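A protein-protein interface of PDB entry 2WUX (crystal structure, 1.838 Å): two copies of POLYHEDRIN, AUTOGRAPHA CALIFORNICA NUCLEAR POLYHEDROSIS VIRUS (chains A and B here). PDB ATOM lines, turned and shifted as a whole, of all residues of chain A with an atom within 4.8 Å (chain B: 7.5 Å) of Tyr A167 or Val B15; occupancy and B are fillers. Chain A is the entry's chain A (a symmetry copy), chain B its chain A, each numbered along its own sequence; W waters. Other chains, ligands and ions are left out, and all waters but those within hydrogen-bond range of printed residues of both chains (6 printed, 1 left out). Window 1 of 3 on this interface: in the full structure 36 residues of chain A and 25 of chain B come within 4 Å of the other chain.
Of the 16 printed residues of chain A, 8 touch a printed residue of chain B.
Of the 14 printed residues of chain B, 9 touch a printed residue of chain A.
Among the printed residues, 19 pairs touch across the chains.
Among the printed residues, no Asp or Glu carboxylate lies within 4 Å of a Lys or Arg side-chain nitrogen of the other chain.
Val B15 touches five residues of chain A.
Printed residues of chain B within 4 Å of Ile A169: Val B15 (3.9 Å).
Printed residues of chain A within 4 Å of Lys B231: Gln A138 (3.5 Å) and His A139 (2.8 Å).
Printed residues of chain A within 4 Å of Tyr B16: Ser A170 (3.6 Å).
Of the printed residues of chain A, Arg B12 touches Arg A168 (3.8 Å).
Printed residues of chain B within 4 Å of Glu A166: Thr B13 (3.5 Å).
Leu B54 touches none of the printed residues of chain A.
The nearest residue of chain B that does not touch Tyr A167 is Thr B13 (4.3 Å).
The nearest printed residue of chain A that does not touch Val B15 is Ser A159 (5.3 Å).
The nearest printed residue of chain B that does not touch Ser A159 is Thr B13 (5.1 Å).
Water W4 bridges the side-chain hydroxyl of Ser A159 and the side-chain hydroxyl of Thr B13.
Water W2 lies within hydrogen-bond range of the backbone carbonyl oxygen of Ser A170, the backbone carbonyl oxygen of Val B15 and the backbone NH of Asp B17.
Water W6 lies within hydrogen-bond range of O of Glu A166, O of Thr B13 and NE of Arg A168.
Water W3 lies within hydrogen-bond range of the side-chain hydroxyl (OG1) of Thr B13 and the backbone carbonyl oxygen (O) of Glu A166.
Water W5 lies within hydrogen-bond range of the backbone NH (N) of Asn B18 (2.8 Å), a ring nitrogen (NE2) of His A139 (2.8 Å) and the backbone NH (N) of Asp B17 (3.5 Å).
Water W1 lies within hydrogen-bond range of the guanidinium group of Arg A168 (3.0 Å) and the side-chain hydroxyl of Tyr B14 (3.5 Å).
O of Tyr A167 sits at hydrogen-bond distance from N of Val A122.
The side-chain carboxylate of Glu A166 is in salt-bridge range of the guanidinium group of Arg A168 (2.7 Å).
O of Ala A137 sits at hydrogen-bond distance from N of Ser A159 (2.8 Å).
The side-chain amino group (NZ) of Lys B231 is in hydrogen-bond range of the side-chain amide oxygen (OD1) of Asn B18 (2.7 Å).
The backbone carbonyl oxygen (O) of Tyr B14 sits at hydrogen-bond distance from the backbone NH (N) of Tyr B21, 2.8 Å away.
O of Ile A169 is in hydrogen-bond range of N of Leu A120 (2.8 Å).
No position is printed for both chains.
NH1 of Arg A168 lies within hydrogen-bond range of OH of Tyr B14 (2.8 Å).
The backbone NH (N) of Val B15 sits at hydrogen-bond distance from the backbone carbonyl oxygen (O) of Arg A168.
The side-chain amide oxygen of Gln A138 is in hydrogen-bond range of the side-chain hydroxyl of Tyr B20 (2.8 Å).
O of Val B15 sits at hydrogen-bond distance from N of Ser A170 (3.0 Å).
OG1 of Thr B13 lies within hydrogen-bond range of O of Glu A166 (3.5 Å).
NZ of Lys B231 sits at hydrogen-bond distance from O of His A139 (2.8 Å).
Among the printed residues, merely in contact across the chains: His A139 with Val B15 (3.3 Å), Tyr A167 with Val B15 (3.5 Å), Gln A138 with Lys B231 (3.5 Å), Tyr A167 with Tyr B20 (3.5 Å), Ser A159 with Pro B63 (3.6 Å), Ser A170 with Tyr B16 (3.6 Å), Ser A159 with Tyr B20 (3.7 Å), Arg A168 with Thr B13 (3.7 Å), His A139 with Tyr B20 (3.7 Å), Gln A138 with Pro B63 (3.7 Å), His A139 with Asn B18 (3.8 Å), Arg A168 with Arg B12 (3.8 Å) and Ile A169 with Val B15 (3.9 Å).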
ATOM      1  N   LEU A 120      13.705   2.798  35.077  1.00  0.00           N
ATOM      2  CA  LEU A 120      13.596   4.126  35.649  1.00  0.00           C
ATOM      3  C   LEU A 120      12.336   4.690  35.015  1.00  0.00           C
ATOM      4  O   LEU A 120      12.261   4.797  33.786  1.00  0.00           O
ATOM      5  CB  LEU A 120      14.813   4.976  35.264  1.00  0.00           C
ATOM      6  CG  LEU A 120      14.995   6.371  35.891  1.00  0.00           C
ATOM      7  CD1 LEU A 120      13.907   7.310  35.420  1.00  0.00           C
ATOM      8  CD2 LEU A 120      15.033   6.322  37.403  1.00  0.00           C
ATOM      9  N   VAL A 121      11.337   5.020  35.830  1.00  0.00           N
ATOM     10  CA  VAL A 121      10.093   5.580  35.307  1.00  0.00           C
ATOM     11  C   VAL A 121       9.957   7.044  35.691  1.00  0.00           C
ATOM     12  O   VAL A 121      10.085   7.408  36.862  1.00  0.00           O
ATOM     13  CB  VAL A 121       8.868   4.813  35.844  1.00  0.00           C
ATOM     14  CG1 VAL A 121       7.561   5.481  35.384  1.00  0.00           C
ATOM     15  CG2 VAL A 121       8.939   3.364  35.421  1.00  0.00           C
ATOM     16  N   VAL A 122       9.687   7.893  34.708  1.00  0.00           N
ATOM     17  CA  VAL A 122       9.451   9.295  35.026  1.00  0.00           C
ATOM     18  C   VAL A 122       8.007   9.578  34.680  1.00  0.00           C
ATOM     19  O   VAL A 122       7.609   9.453  33.526  1.00  0.00           O
ATOM     20  CB  VAL A 122      10.355  10.252  34.234  1.00  0.00           C
ATOM     21  CG1 VAL A 122      10.152  11.704  34.716  1.00  0.00           C
ATOM     22  CG2 VAL A 122      11.824   9.832  34.342  1.00  0.00           C
ATOM     23  N   MET A 124       4.983  12.446  34.738  1.00  0.00           N
ATOM     24  CA  MET A 124       4.939  13.895  34.666  1.00  0.00           C
ATOM     25  C   MET A 124       3.500  14.373  34.584  1.00  0.00           C
ATOM     26  O   MET A 124       2.659  13.714  33.983  1.00  0.00           O
ATOM     27  CB  MET A 124       5.713  14.387  33.443  1.00  0.00           C
ATOM     28  CG  MET A 124       5.376  13.642  32.156  1.00  0.00           C
ATOM     29  SD  MET A 124       6.849  13.353  31.109  1.00  0.00           S
ATOM     30  CE  MET A 124       7.548  11.913  31.922  1.00  0.00           C
ATOM     31  N   ALA A 137      11.016  13.776  25.981  1.00  0.00           N
ATOM     32  CA  ALA A 137      12.041  13.268  26.867  1.00  0.00           C
ATOM     33  C   ALA A 137      13.272  12.767  26.118  1.00  0.00           C
ATOM     34  O   ALA A 137      13.198  12.431  24.940  1.00  0.00           O
ATOM     35  CB  ALA A 137      11.456  12.158  27.752  1.00  0.00           C
ATOM     36  N   GLN A 138      14.403  12.768  26.811  1.00  0.00           N
ATOM     37  CA  GLN A 138      15.602  12.059  26.361  1.00  0.00           C
ATOM     38  C   GLN A 138      16.443  11.658  27.558  1.00  0.00           C
ATOM     39  O   GLN A 138      16.458  12.331  28.597  1.00  0.00           O
ATOM     40  CB  GLN A 138      16.444  12.857  25.363  1.00  0.00           C
ATOM     41  CG  GLN A 138      17.462  11.971  24.602  1.00  0.00           C
ATOM     42  CD  GLN A 138      16.835  10.695  23.984  1.00  0.00           C
ATOM     43  OE1 GLN A 138      16.710   9.656  24.643  1.00  0.00           O
ATOM     44  NE2 GLN A 138      16.459  10.779  22.711  1.00  0.00           N
ATOM     45  N   HIS A 139      17.126  10.536  27.414  1.00  0.00           N
ATOM     46  CA  HIS A 139      17.897   9.992  28.510  1.00  0.00           C
ATOM     47  C   HIS A 139      19.273   9.591  28.001  1.00  0.00           C
ATOM     48  O   HIS A 139      19.552   9.604  26.797  1.00  0.00           O
ATOM     49  CB  HIS A 139      17.186   8.753  29.062  1.00  0.00           C
ATOM     50  CG  HIS A 139      17.232   7.592  28.123  1.00  0.00           C
ATOM     51  ND1 HIS A 139      16.354   7.455  27.071  1.00  0.00           N
ATOM     52  CD2 HIS A 139      18.107   6.565  28.020  1.00  0.00           C
ATOM     53  CE1 HIS A 139      16.661   6.368  26.383  1.00  0.00           C
ATOM     54  NE2 HIS A 139      17.722   5.808  26.940  1.00  0.00           N
ATOM     55  N   SER A 159      12.372  11.919  22.268  1.00  0.00           N
ATOM     56  CA  SER A 159      11.312  10.929  22.341  1.00  0.00           C
ATOM     57  C   SER A 159       9.996  11.611  22.708  1.00  0.00           C
ATOM     58  O   SER A 159       9.943  12.438  23.625  1.00  0.00           O
ATOM     59  CB  SER A 159      11.651   9.840  23.365  1.00  0.00           C
ATOM     60  OG  SER A 159      10.598   8.888  23.435  1.00  0.00           O
ATOM     61  N   VAL A 161       6.548  11.518  24.472  1.00  0.00           N
ATOM     62  CA  VAL A 161       5.887  10.778  25.533  1.00  0.00           C
ATOM     63  C   VAL A 161       4.400  10.643  25.208  1.00  0.00           C
ATOM     64  O   VAL A 161       3.749  11.611  24.787  1.00  0.00           O
ATOM     65  CB  VAL A 161       6.054  11.481  26.886  1.00  0.00           C
ATOM     66  CG1 VAL A 161       5.374  10.694  27.987  1.00  0.00           C
ATOM     67  CG2 VAL A 161       7.547  11.713  27.200  1.00  0.00           C
ATOM     68  N   ASN A 165       1.622   9.907  30.029  1.00  0.00           N
ATOM     69  CA  ASN A 165       2.569  10.857  30.602  1.00  0.00           C
ATOM     70  C   ASN A 165       3.675  10.193  31.406  1.00  0.00           C
ATOM     71  O   ASN A 165       4.083  10.694  32.462  1.00  0.00           O
ATOM     72  CB  ASN A 165       1.838  11.904  31.448  1.00  0.00           C
ATOM     73  CG  ASN A 165       0.973  12.831  30.610  1.00  0.00           C
ATOM     74  OD1 ASN A 165       1.125  12.922  29.381  1.00  0.00           O
ATOM     75  ND2 ASN A 165       0.063  13.530  31.270  1.00  0.00           N
ATOM     76  N   GLU A 166       4.155   9.065  30.905  1.00  0.00           N
ATOM     77  CA  GLU A 166       5.252   8.353  31.547  1.00  0.00           C
ATOM     78  C   GLU A 166       6.325   7.941  30.563  1.00  0.00           C
ATOM     79  O   GLU A 166       6.037   7.433  29.485  1.00  0.00           O
ATOM     80  CB  GLU A 166       4.753   7.117  32.300  1.00  0.00           C
ATOM     81  CG  GLU A 166       4.134   7.469  33.632  1.00  0.00           C
ATOM     82  CD  GLU A 166       3.949   6.277  34.555  1.00  0.00           C
ATOM     83  OE1 GLU A 166       4.213   5.125  34.139  1.00  0.00           O
ATOM     84  OE2 GLU A 166       3.528   6.510  35.706  1.00  0.00           O
ATOM     85  N   TYR A 167       7.567   8.169  30.965  1.00  0.00           N
ATOM     86  CA  TYR A 167       8.729   7.737  30.210  1.00  0.00           C
ATOM     87  C   TYR A 167       9.387   6.606  30.995  1.00  0.00           C
ATOM     88  O   TYR A 167       9.749   6.778  32.166  1.00  0.00           O
ATOM     89  CB  TYR A 167       9.686   8.914  30.071  1.00  0.00           C
ATOM     90  CG  TYR A 167      10.794   8.727  29.069  1.00  0.00           C
ATOM     91  CD1 TYR A 167      12.123   8.822  29.455  1.00  0.00           C
ATOM     92  CD2 TYR A 167      10.515   8.480  27.728  1.00  0.00           C
ATOM     93  CE1 TYR A 167      13.136   8.686  28.552  1.00  0.00           C
ATOM     94  CE2 TYR A 167      11.536   8.328  26.810  1.00  0.00           C
ATOM     95  CZ  TYR A 167      12.848   8.435  27.234  1.00  0.00           C
ATOM     96  OH  TYR A 167      13.888   8.298  26.338  1.00  0.00           O
ATOM     97  N   ARG A 168       9.529   5.445  30.362  1.00  0.00           N
ATOM     98  CA  ARG A 168       9.992   4.252  31.070  1.00  0.00           C
ATOM     99  C   ARG A 168      11.248   3.715  30.420  1.00  0.00           C
ATOM    100  O   ARG A 168      11.209   3.280  29.280  1.00  0.00           O
ATOM    101  CB  ARG A 168       8.900   3.172  31.054  1.00  0.00           C
ATOM    102  CG  ARG A 168       7.601   3.657  31.658  1.00  0.00           C
ATOM    103  CD  ARG A 168       6.453   2.687  31.461  1.00  0.00           C
ATOM    104  NE  ARG A 168       5.259   3.183  32.150  1.00  0.00           N
ATOM    105  CZ  ARG A 168       4.064   2.612  32.080  1.00  0.00           C
ATOM    106  NH1 ARG A 168       3.904   1.520  31.353  1.00  0.00           N
ATOM    107  NH2 ARG A 168       3.029   3.130  32.732  1.00  0.00           N
ATOM    108  N   ILE A 169      12.347   3.722  31.167  1.00  0.00           N
ATOM    109  CA  ILE A 169      13.659   3.379  30.638  1.00  0.00           C
ATOM    110  C   ILE A 169      14.172   2.084  31.258  1.00  0.00           C
ATOM    111  O   ILE A 169      14.390   2.031  32.454  1.00  0.00           O
ATOM    112  CB  ILE A 169      14.686   4.466  31.004  1.00  0.00           C
ATOM    113  CG1 ILE A 169      14.180   5.849  30.586  1.00  0.00           C
ATOM    114  CG2 ILE A 169      16.031   4.160  30.380  1.00  0.00           C
ATOM    115  CD1 ILE A 169      14.977   6.989  31.200  1.00  0.00           C
ATOM    116  N   SER A 170      14.374   1.054  30.445  1.00  0.00           N
ATOM    117  CA  SER A 170      15.033  -0.165  30.923  1.00  0.00           C
ATOM    118  C   SER A 170      16.495   0.088  31.262  1.00  0.00           C
ATOM    119  O   SER A 170      17.239   0.614  30.445  1.00  0.00           O
ATOM    120  CB  SER A 170      14.979  -1.257  29.870  1.00  0.00           C
ATOM    121  OG  SER A 170      15.875  -2.291  30.230  1.00  0.00           O
ATOM    122  N   VAL A 208      18.129  11.741  32.835  1.00  0.00           N
ATOM    123  CA  VAL A 208      16.946  11.917  32.028  1.00  0.00           C
ATOM    124  C   VAL A 208      16.635  13.394  31.991  1.00  0.00           C
ATOM    125  O   VAL A 208      16.817  14.096  32.984  1.00  0.00           O
ATOM    126  CB  VAL A 208      15.728  11.162  32.628  1.00  0.00           C
ATOM    127  CG1 VAL A 208      14.541  11.209  31.656  1.00  0.00           C
ATOM    128  CG2 VAL A 208      16.102   9.729  32.937  1.00  0.00           C
ATOM    129  N   ARG B  12       1.572   4.694  25.651  1.00  0.00           N
ATOM    130  CA  ARG B  12       2.671   4.468  26.575  1.00  0.00           C
ATOM    131  C   ARG B  12       3.925   4.093  25.805  1.00  0.00           C
ATOM    132  O   ARG B  12       3.860   3.478  24.738  1.00  0.00           O
ATOM    133  CB  ARG B  12       2.312   3.414  27.626  1.00  0.00           C
ATOM    134  CG  ARG B  12       2.469   1.979  27.188  1.00  0.00           C
ATOM    135  CD  ARG B  12       1.830   1.044  28.216  1.00  0.00           C
ATOM    136  NE  ARG B  12       0.375   1.015  28.089  1.00  0.00           N
ATOM    137  CZ  ARG B  12      -0.292   0.079  27.422  1.00  0.00           C
ATOM    138  NH1 ARG B  12      -1.615   0.127  27.344  1.00  0.00           N
ATOM    139  NH2 ARG B  12       0.366  -0.909  26.833  1.00  0.00           N
ATOM    140  N   THR B  13       5.068   4.496  26.338  1.00  0.00           N
ATOM    141  CA  THR B  13       6.329   4.284  25.646  1.00  0.00           C
ATOM    142  C   THR B  13       7.335   3.608  26.567  1.00  0.00           C
ATOM    143  O   THR B  13       7.285   3.779  27.790  1.00  0.00           O
ATOM    144  CB  THR B  13       6.920   5.622  25.152  1.00  0.00           C
ATOM    145  OG1 THR B  13       7.029   6.526  26.254  1.00  0.00           O
ATOM    146  CG2 THR B  13       6.023   6.250  24.078  1.00  0.00           C
ATOM    147  N   TYR B  14       8.239   2.845  25.964  1.00  0.00           N
ATOM    148  CA  TYR B  14       9.345   2.212  26.660  1.00  0.00           C
ATOM    149  C   TYR B  14      10.602   2.406  25.825  1.00  0.00           C
ATOM    150  O   TYR B  14      10.524   2.493  24.590  1.00  0.00           O
ATOM    151  CB  TYR B  14       9.100   0.704  26.799  1.00  0.00           C
ATOM    152  CG  TYR B  14       8.032   0.304  27.783  1.00  0.00           C
ATOM    153  CD1 TYR B  14       8.351   0.045  29.112  1.00  0.00           C
ATOM    154  CD2 TYR B  14       6.707   0.151  27.383  1.00  0.00           C
ATOM    155  CE1 TYR B  14       7.383  -0.334  30.020  1.00  0.00           C
ATOM    156  CE2 TYR B  14       5.729  -0.231  28.288  1.00  0.00           C
ATOM    157  CZ  TYR B  14       6.076  -0.474  29.601  1.00  0.00           C
ATOM    158  OH  TYR B  14       5.112  -0.859  30.510  1.00  0.00           O
ATOM    159  N   VAL B  15      11.757   2.460  26.488  1.00  0.00           N
ATOM    160  CA  VAL B  15      13.043   2.445  25.789  1.00  0.00           C
ATOM    161  C   VAL B  15      13.887   1.265  26.249  1.00  0.00           C
ATOM    162  O   VAL B  15      14.129   1.096  27.458  1.00  0.00           O
ATOM    163  CB  VAL B  15      13.880   3.712  26.038  1.00  0.00           C
ATOM    164  CG1 VAL B  15      15.026   3.776  25.031  1.00  0.00           C
ATOM    165  CG2 VAL B  15      13.023   4.950  25.955  1.00  0.00           C
ATOM    166  N   TYR B  16      14.320   0.452  25.284  1.00  0.00           N
ATOM    167  CA  TYR B  16      15.268  -0.638  25.527  1.00  0.00           C
ATOM    168  C   TYR B  16      16.553  -0.434  24.719  1.00  0.00           C
ATOM    169  O   TYR B  16      16.554  -0.603  23.495  1.00  0.00           O
ATOM    170  CB  TYR B  16      14.668  -1.977  25.112  1.00  0.00           C
ATOM    171  CG  TYR B  16      13.599  -2.524  26.020  1.00  0.00           C
ATOM    172  CD1 TYR B  16      13.929  -3.358  27.080  1.00  0.00           C
ATOM    173  CD2 TYR B  16      12.257  -2.242  25.798  1.00  0.00           C
ATOM    174  CE1 TYR B  16      12.956  -3.886  27.903  1.00  0.00           C
ATOM    175  CE2 TYR B  16      11.269  -2.768  26.616  1.00  0.00           C
ATOM    176  CZ  TYR B  16      11.630  -3.586  27.669  1.00  0.00           C
ATOM    177  OH  TYR B  16      10.672  -4.114  28.496  1.00  0.00           O
ATOM    178  N   ASP B  17      17.642  -0.085  25.401  1.00  0.00           N
ATOM    179  CA  ASP B  17      18.929   0.123  24.743  1.00  0.00           C
ATOM    180  C   ASP B  17      18.760   0.983  23.492  1.00  0.00           C
ATOM    181  O   ASP B  17      19.141   0.578  22.389  1.00  0.00           O
ATOM    182  CB  ASP B  17      19.574  -1.219  24.384  1.00  0.00           C
ATOM    183  CG  ASP B  17      21.046  -1.085  24.022  1.00  0.00           C
ATOM    184  OD1 ASP B  17      21.689  -2.123  23.750  1.00  0.00           O
ATOM    185  OD2 ASP B  17      21.560   0.055  24.013  1.00  0.00           O
ATOM    186  N   ASN B  18      18.174   2.164  23.679  1.00  0.00           N
ATOM    187  CA  ASN B  18      17.937   3.111  22.588  1.00  0.00           C
ATOM    188  C   ASN B  18      17.031   2.625  21.446  1.00  0.00           C
ATOM    189  O   ASN B  18      16.992   3.238  20.371  1.00  0.00           O
ATOM    190  CB  ASN B  18      19.262   3.670  22.057  1.00  0.00           C
ATOM    191  CG  ASN B  18      19.836   4.744  22.963  1.00  0.00           C
ATOM    192  OD1 ASN B  18      19.107   5.610  23.456  1.00  0.00           O
ATOM    193  ND2 ASN B  18      21.143   4.691  23.193  1.00  0.00           N
ATOM    194  N   LYS B  19      16.326   1.518  21.680  1.00  0.00           N
ATOM    195  CA  LYS B  19      15.183   1.138  20.857  1.00  0.00           C
ATOM    196  C   LYS B  19      13.917   1.614  21.558  1.00  0.00           C
ATOM    197  O   LYS B  19      13.676   1.273  22.723  1.00  0.00           O
ATOM    198  CB  LYS B  19      15.111  -0.375  20.659  1.00  0.00           C
ATOM    199  CG  LYS B  19      16.274  -0.984  19.897  1.00  0.00           C
ATOM    200  CD  LYS B  19      16.083  -2.492  19.768  1.00  0.00           C
ATOM    201  CE  LYS B  19      17.342  -3.178  19.267  1.00  0.00           C
ATOM    202  NZ  LYS B  19      17.121  -4.635  19.037  1.00  0.00           N
ATOM    203  N   TYR B  20      13.118   2.410  20.855  1.00  0.00           N
ATOM    204  CA  TYR B  20      11.905   2.980  21.421  1.00  0.00           C
ATOM    205  C   TYR B  20      10.673   2.206  20.974  1.00  0.00           C
ATOM    206  O   TYR B  20      10.571   1.813  19.811  1.00  0.00           O
ATOM    207  CB  TYR B  20      11.776   4.442  21.009  1.00  0.00           C
ATOM    208  CG  TYR B  20      12.929   5.277  21.507  1.00  0.00           C
ATOM    209  CD1 TYR B  20      12.806   6.055  22.658  1.00  0.00           C
ATOM    210  CD2 TYR B  20      14.150   5.271  20.842  1.00  0.00           C
ATOM    211  CE1 TYR B  20      13.870   6.813  23.125  1.00  0.00           C
ATOM    212  CE2 TYR B  20      15.218   6.023  21.302  1.00  0.00           C
ATOM    213  CZ  TYR B  20      15.074   6.793  22.439  1.00  0.00           C
ATOM    214  OH  TYR B  20      16.141   7.537  22.885  1.00  0.00           O
ATOM    215  N   TYR B  21       9.742   2.007  21.902  1.00  0.00           N
ATOM    216  CA  TYR B  21       8.548   1.206  21.653  1.00  0.00           C
ATOM    217  C   TYR B  21       7.309   1.965  22.073  1.00  0.00           C
ATOM    218  O   TYR B  21       7.356   2.772  22.999  1.00  0.00           O
ATOM    219  CB  TYR B  21       8.593  -0.080  22.464  1.00  0.00           C
ATOM    220  CG  TYR B  21       9.696  -1.033  22.085  1.00  0.00           C
ATOM    221  CD1 TYR B  21       9.412  -2.207  21.399  1.00  0.00           C
ATOM    222  CD2 TYR B  21      11.017  -0.770  22.426  1.00  0.00           C
ATOM    223  CE1 TYR B  21      10.413  -3.096  21.061  1.00  0.00           C
ATOM    224  CE2 TYR B  21      12.026  -1.648  22.092  1.00  0.00           C
ATOM    225  CZ  TYR B  21      11.716  -2.810  21.409  1.00  0.00           C
ATOM    226  OH  TYR B  21      12.713  -3.685  21.070  1.00  0.00           O
ATOM    227  N   LEU B  54       3.444  -4.172  22.233  1.00  0.00           N
ATOM    228  CA  LEU B  54       4.253  -3.032  21.802  1.00  0.00           C
ATOM    229  C   LEU B  54       4.818  -3.231  20.406  1.00  0.00           C
ATOM    230  O   LEU B  54       5.101  -4.359  19.987  1.00  0.00           O
ATOM    231  CB  LEU B  54       5.450  -2.834  22.745  1.00  0.00           C
ATOM    232  CG  LEU B  54       5.212  -2.696  24.245  1.00  0.00           C
ATOM    233  CD1 LEU B  54       6.527  -2.375  24.935  1.00  0.00           C
ATOM    234  CD2 LEU B  54       4.175  -1.622  24.527  1.00  0.00           C
ATOM    235  N   PRO B  63      13.686   8.789  17.740  1.00  0.00           N
ATOM    236  CA  PRO B  63      14.528   9.805  18.387  1.00  0.00           C
ATOM    237  C   PRO B  63      15.984   9.764  17.927  1.00  0.00           C
ATOM    238  O   PRO B  63      16.487   8.727  17.491  1.00  0.00           O
ATOM    239  CB  PRO B  63      14.438   9.442  19.866  1.00  0.00           C
ATOM    240  CG  PRO B  63      13.064   8.772  20.000  1.00  0.00           C
ATOM    241  CD  PRO B  63      12.871   8.033  18.707  1.00  0.00           C
ATOM    242  N   MET B 116      24.060   6.447  19.356  1.00  0.00           N
ATOM    243  CA  MET B 116      23.092   5.458  19.832  1.00  0.00           C
ATOM    244  C   MET B 116      23.277   4.129  19.112  1.00  0.00           C
ATOM    245  O   MET B 116      23.096   3.062  19.701  1.00  0.00           O
ATOM    246  CB  MET B 116      21.669   5.946  19.573  1.00  0.00           C
ATOM    247  CG  MET B 116      21.314   7.265  20.232  1.00  0.00           C
ATOM    248  SD  MET B 116      19.891   8.014  19.412  1.00  0.00           S
ATOM    249  CE  MET B 116      18.686   6.703  19.607  1.00  0.00           C
ATOM    250  N   LYS B 231      22.436  11.150  19.492  1.00  0.00           N
ATOM    251  CA  LYS B 231      21.639  11.855  20.477  1.00  0.00           C
ATOM    252  C   LYS B 231      22.487  13.012  20.985  1.00  0.00           C
ATOM    253  O   LYS B 231      23.534  12.791  21.605  1.00  0.00           O
ATOM    254  CB  LYS B 231      21.306  10.873  21.595  1.00  0.00           C
ATOM    255  CG  LYS B 231      20.484  11.404  22.718  1.00  0.00           C
ATOM    256  CD  LYS B 231      20.460  10.368  23.854  1.00  0.00           C
ATOM    257  CE  LYS B 231      19.975   9.005  23.371  1.00  0.00           C
ATOM    258  NZ  LYS B 231      19.890   8.013  24.500  1.00  0.00           N
HETATM  259  O   HOH W   1       1.711  -0.512  31.024  1.00  0.00           O
HETATM  260  O   HOH W   2      17.029   1.442  27.967  1.00  0.00           O
HETATM  261  O   HOH W   3       4.563   7.239  27.189  1.00  0.00           O
HETATM  262  O   HOH W   4       8.362   8.423  24.716  1.00  0.00           O
HETATM  263  O   HOH W   5      18.457   3.175  26.266  1.00  0.00           O
HETATM  264  O   HOH W   6       5.154   4.870  29.274  1.00  0.00           O
